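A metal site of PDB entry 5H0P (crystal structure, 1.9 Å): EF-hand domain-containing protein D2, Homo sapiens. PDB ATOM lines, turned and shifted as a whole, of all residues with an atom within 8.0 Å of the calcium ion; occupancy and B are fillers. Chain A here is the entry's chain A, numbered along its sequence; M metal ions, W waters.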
ATOM      1  N   PHE A  37       9.509   1.556 -14.772  1.00  0.00           N
ATOM      2  CA  PHE A  37       9.844   2.947 -15.036  1.00  0.00           C
ATOM      3  C   PHE A  37       9.932   3.762 -13.740  1.00  0.00           C
ATOM      4  O   PHE A  37      10.928   4.472 -13.508  1.00  0.00           O
ATOM      5  CB  PHE A  37       8.832   3.568 -16.015  1.00  0.00           C
ATOM      6  CG  PHE A  37       9.170   4.964 -16.432  1.00  0.00           C
ATOM      7  CD1 PHE A  37       8.747   6.039 -15.685  1.00  0.00           C
ATOM      8  CD2 PHE A  37       9.929   5.200 -17.575  1.00  0.00           C
ATOM      9  CE1 PHE A  37       9.074   7.340 -16.054  1.00  0.00           C
ATOM     10  CE2 PHE A  37      10.251   6.508 -17.953  1.00  0.00           C
ATOM     11  CZ  PHE A  37       9.818   7.569 -17.192  1.00  0.00           C
ATOM     12  N   TYR A  40      12.993   3.106 -11.341  1.00  0.00           N
ATOM     13  CA  TYR A  40      14.299   3.678 -11.661  1.00  0.00           C
ATOM     14  C   TYR A  40      14.344   5.190 -11.897  1.00  0.00           C
ATOM     15  O   TYR A  40      15.434   5.773 -12.008  1.00  0.00           O
ATOM     16  CB  TYR A  40      14.958   2.889 -12.795  1.00  0.00           C
ATOM     17  CG  TYR A  40      15.274   1.472 -12.384  1.00  0.00           C
ATOM     18  CD1 TYR A  40      16.400   1.186 -11.653  1.00  0.00           C
ATOM     19  CD2 TYR A  40      14.418   0.421 -12.718  1.00  0.00           C
ATOM     20  CE1 TYR A  40      16.694  -0.107 -11.267  1.00  0.00           C
ATOM     21  CE2 TYR A  40      14.699  -0.875 -12.336  1.00  0.00           C
ATOM     22  CZ  TYR A  40      15.843  -1.130 -11.611  1.00  0.00           C
ATOM     23  OH  TYR A  40      16.141  -2.415 -11.220  1.00  0.00           O
ATOM     24  N   ASP A  41      13.175   5.825 -11.938  1.00  0.00           N
ATOM     25  CA  ASP A  41      13.104   7.289 -11.905  1.00  0.00           C
ATOM     26  C   ASP A  41      13.368   7.759 -10.479  1.00  0.00           C
ATOM     27  O   ASP A  41      12.432   7.999  -9.705  1.00  0.00           O
ATOM     28  CB  ASP A  41      11.750   7.793 -12.428  1.00  0.00           C
ATOM     29  CG  ASP A  41      11.634   9.323 -12.382  1.00  0.00           C
ATOM     30  OD1 ASP A  41      12.654  10.013 -12.162  1.00  0.00           O
ATOM     31  OD2 ASP A  41      10.506   9.846 -12.577  1.00  0.00           O
ATOM     32  N   ALA A  42      14.647   7.897 -10.151  1.00  0.00           N
ATOM     33  CA  ALA A  42      15.061   8.195  -8.782  1.00  0.00           C
ATOM     34  C   ALA A  42      14.536   9.547  -8.291  1.00  0.00           C
ATOM     35  O   ALA A  42      14.270   9.708  -7.106  1.00  0.00           O
ATOM     36  CB  ALA A  42      16.580   8.119  -8.655  1.00  0.00           C
ATOM     37  N   GLY A  43      14.381  10.502  -9.201  1.00  0.00           N
ATOM     38  CA  GLY A  43      14.015  11.856  -8.818  1.00  0.00           C
ATOM     39  C   GLY A  43      12.539  12.200  -8.906  1.00  0.00           C
ATOM     40  O   GLY A  43      12.145  13.327  -8.608  1.00  0.00           O
ATOM     41  N   ARG A  44      11.726  11.217  -9.313  1.00  0.00           N
ATOM     42  CA  ARG A  44      10.277  11.382  -9.417  1.00  0.00           C
ATOM     43  C   ARG A  44       9.885  12.525 -10.357  1.00  0.00           C
ATOM     44  O   ARG A  44       8.844  13.155 -10.163  1.00  0.00           O
ATOM     45  CB  ARG A  44       9.673  11.623  -8.034  1.00  0.00           C
ATOM     46  CG  ARG A  44      10.091  10.602  -6.995  1.00  0.00           C
ATOM     47  CD  ARG A  44       9.659   9.211  -7.403  1.00  0.00           C
ATOM     48  NE  ARG A  44      10.149   8.177  -6.503  1.00  0.00           N
ATOM     49  CZ  ARG A  44       9.923   6.882  -6.659  1.00  0.00           C
ATOM     50  NH1 ARG A  44       9.214   6.453  -7.688  1.00  0.00           N
ATOM     51  NH2 ARG A  44      10.414   6.011  -5.785  1.00  0.00           N
ATOM     52  N   ASP A  45      10.719  12.793 -11.354  1.00  0.00           N
ATOM     53  CA  ASP A  45      10.444  13.901 -12.273  1.00  0.00           C
ATOM     54  C   ASP A  45       9.642  13.444 -13.485  1.00  0.00           C
ATOM     55  O   ASP A  45       9.185  14.262 -14.292  1.00  0.00           O
ATOM     56  CB  ASP A  45      11.727  14.643 -12.701  1.00  0.00           C
ATOM     57  CG  ASP A  45      12.623  13.818 -13.602  1.00  0.00           C
ATOM     58  OD1 ASP A  45      12.472  12.575 -13.626  1.00  0.00           O
ATOM     59  OD2 ASP A  45      13.494  14.405 -14.276  1.00  0.00           O
ATOM     60  N   GLY A  46       9.472  12.133 -13.596  1.00  0.00           N
ATOM     61  CA  GLY A  46       8.707  11.535 -14.674  1.00  0.00           C
ATOM     62  C   GLY A  46       9.551  11.113 -15.857  1.00  0.00           C
ATOM     63  O   GLY A  46       9.023  10.798 -16.922  1.00  0.00           O
ATOM     64  N   PHE A  47      10.867  11.131 -15.687  1.00  0.00           N
ATOM     65  CA  PHE A  47      11.779  10.765 -16.762  1.00  0.00           C
ATOM     66  C   PHE A  47      12.838   9.831 -16.268  1.00  0.00           C
ATOM     67  O   PHE A  47      13.120   9.763 -15.067  1.00  0.00           O
ATOM     68  CB  PHE A  47      12.426  12.010 -17.358  1.00  0.00           C
ATOM     69  CG  PHE A  47      11.441  12.963 -17.934  1.00  0.00           C
ATOM     70  CD1 PHE A  47      10.997  12.807 -19.236  1.00  0.00           C
ATOM     71  CD2 PHE A  47      10.925  13.999 -17.163  1.00  0.00           C
ATOM     72  CE1 PHE A  47      10.086  13.673 -19.768  1.00  0.00           C
ATOM     73  CE2 PHE A  47      10.005  14.869 -17.695  1.00  0.00           C
ATOM     74  CZ  PHE A  47       9.574  14.716 -18.992  1.00  0.00           C
ATOM     75  N   ILE A  48      13.419   9.074 -17.202  1.00  0.00           N
ATOM     76  CA  ILE A  48      14.636   8.375 -16.904  1.00  0.00           C
ATOM     77  C   ILE A  48      15.736   9.068 -17.693  1.00  0.00           C
ATOM     78  O   ILE A  48      15.694   9.067 -18.928  1.00  0.00           O
ATOM     79  CB  ILE A  48      14.584   6.901 -17.334  1.00  0.00           C
ATOM     80  CG1 ILE A  48      13.493   6.162 -16.560  1.00  0.00           C
ATOM     81  CG2 ILE A  48      15.920   6.234 -17.022  1.00  0.00           C
ATOM     82  CD1 ILE A  48      13.760   6.165 -15.103  1.00  0.00           C
ATOM     83  N   ASP A  49      16.681   9.671 -16.983  1.00  0.00           N
ATOM     84  CA  ASP A  49      17.846  10.274 -17.620  1.00  0.00           C
ATOM     85  C   ASP A  49      18.994   9.273 -17.715  1.00  0.00           C
ATOM     86  O   ASP A  49      18.881   8.121 -17.271  1.00  0.00           O
ATOM     87  CB  ASP A  49      18.297  11.578 -16.907  1.00  0.00           C
ATOM     88  CG  ASP A  49      18.625  11.363 -15.427  1.00  0.00           C
ATOM     89  OD1 ASP A  49      19.177  10.305 -15.052  1.00  0.00           O
ATOM     90  OD2 ASP A  49      18.321  12.270 -14.621  1.00  0.00           O
ATOM     91  N   LEU A  50      20.122   9.741 -18.250  1.00  0.00           N
ATOM     92  CA  LEU A  50      21.244   8.853 -18.531  1.00  0.00           C
ATOM     93  C   LEU A  50      21.782   8.205 -17.257  1.00  0.00           C
ATOM     94  O   LEU A  50      22.066   7.007 -17.225  1.00  0.00           O
ATOM     95  CB  LEU A  50      22.357   9.622 -19.241  1.00  0.00           C
ATOM     96  CG  LEU A  50      23.515   8.732 -19.691  1.00  0.00           C
ATOM     97  CD1 LEU A  50      23.848   9.025 -21.136  1.00  0.00           C
ATOM     98  CD2 LEU A  50      24.713   8.911 -18.782  1.00  0.00           C
ATOM     99  N   GLU A  52      20.186   7.731 -14.429  1.00  0.00           N
ATOM    100  CA  GLU A  52      19.186   6.782 -13.954  1.00  0.00           C
ATOM    101  C   GLU A  52      19.212   5.517 -14.780  1.00  0.00           C
ATOM    102  O   GLU A  52      19.031   4.420 -14.257  1.00  0.00           O
ATOM    103  CB  GLU A  52      17.783   7.410 -13.989  1.00  0.00           C
ATOM    104  CG  GLU A  52      17.544   8.380 -12.828  1.00  0.00           C
ATOM    105  CD  GLU A  52      16.379   9.302 -13.080  1.00  0.00           C
ATOM    106  OE1 GLU A  52      16.097   9.579 -14.256  1.00  0.00           O
ATOM    107  OE2 GLU A  52      15.740   9.774 -12.118  1.00  0.00           O
ATOM    108  N   LEU A  53      19.435   5.654 -16.084  1.00  0.00           N
ATOM    109  CA  LEU A  53      19.542   4.467 -16.945  1.00  0.00           C
ATOM    110  C   LEU A  53      20.798   3.655 -16.636  1.00  0.00           C
ATOM    111  O   LEU A  53      20.764   2.419 -16.623  1.00  0.00           O
ATOM    112  CB  LEU A  53      19.481   4.850 -18.437  1.00  0.00           C
ATOM    113  CG  LEU A  53      19.491   3.713 -19.462  1.00  0.00           C
ATOM    114  CD1 LEU A  53      18.248   2.796 -19.325  1.00  0.00           C
ATOM    115  CD2 LEU A  53      19.567   4.274 -20.857  1.00  0.00           C
ATOM    116  N   LYS A  83      16.467  12.321 -22.411  1.00  0.00           N
ATOM    117  CA  LYS A  83      15.975  11.506 -21.326  1.00  0.00           C
ATOM    118  C   LYS A  83      14.703  10.803 -21.792  1.00  0.00           C
ATOM    119  O   LYS A  83      14.143  11.156 -22.819  1.00  0.00           O
ATOM    120  CB  LYS A  83      15.710  12.339 -20.070  1.00  0.00           C
ATOM    121  CG  LYS A  83      14.794  13.552 -20.270  1.00  0.00           C
ATOM    122  CD  LYS A  83      14.595  14.344 -18.978  1.00  0.00           C
ATOM    123  CE  LYS A  83      13.670  15.536 -19.199  1.00  0.00           C
ATOM    124  NZ  LYS A  83      13.394  16.248 -17.938  1.00  0.00           N
ATOM    125  N   LEU A  84      14.270   9.799 -21.040  1.00  0.00           N
ATOM    126  CA  LEU A  84      13.148   8.977 -21.474  1.00  0.00           C
ATOM    127  C   LEU A  84      11.886   9.271 -20.697  1.00  0.00           C
ATOM    128  O   LEU A  84      11.865   9.137 -19.476  1.00  0.00           O
ATOM    129  CB  LEU A  84      13.482   7.484 -21.264  1.00  0.00           C
ATOM    130  CG  LEU A  84      14.726   6.870 -21.893  1.00  0.00           C
ATOM    131  CD1 LEU A  84      14.842   5.406 -21.458  1.00  0.00           C
ATOM    132  CD2 LEU A  84      14.674   6.957 -23.397  1.00  0.00           C
HETATM  133 CA    CA M   1      14.300  11.048 -13.392  1.00  0.00          CA
HETATM  134  O   HOH W   1      15.123  12.737 -15.143  1.00  0.00           O
HETATM  135  O   HOH W   2      15.158  12.896 -11.805  1.00  0.00           O
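Within 4 Å of the calcium ion: Asp 41, Asp 45, Phe 47 and Glu 52.
Water W1 lies within hydrogen-bond range of OD2 of Asp 45 and OD2 of Asp 49.
The calcium ion is bound by the side-chain carboxylate (OD1) of Asp 41 (2.3 Å), the side-chain carboxylate (OE2) of Glu 52 (2.3 Å), the side-chain carboxylate (OD1) of Asp 45 (2.4 Å), the backbone carbonyl oxygen (O) of Phe 47 (2.4 Å), the side-chain carboxylate (OE1) of Glu 52 (2.5 Å), water W1 (2.6 Å) and water W2 (2.6 Å).
N of Gly 43 lies close to OD1 of Asp 41 (3.5 Å).
The side-chain carboxylate of Asp 41 lies close to the backbone NH of Arg 44 (3.2 Å).
OD2 of Asp 41 lies within hydrogen-bond range of N of Gly 46, 2.7 Å away.
The backbone NH of Gly 43 lies close to the side-chain carboxylate of Glu 52, 3.3 Å away.
The backbone NH (N) of Glu 52 lies within hydrogen-bond range of the side-chain carboxylate (OD1) of Asp 49, at 2.8 Å.
The side-chain carboxylate (OE2) of Glu 52 lies close to the backbone NH (N) of Ala 42.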
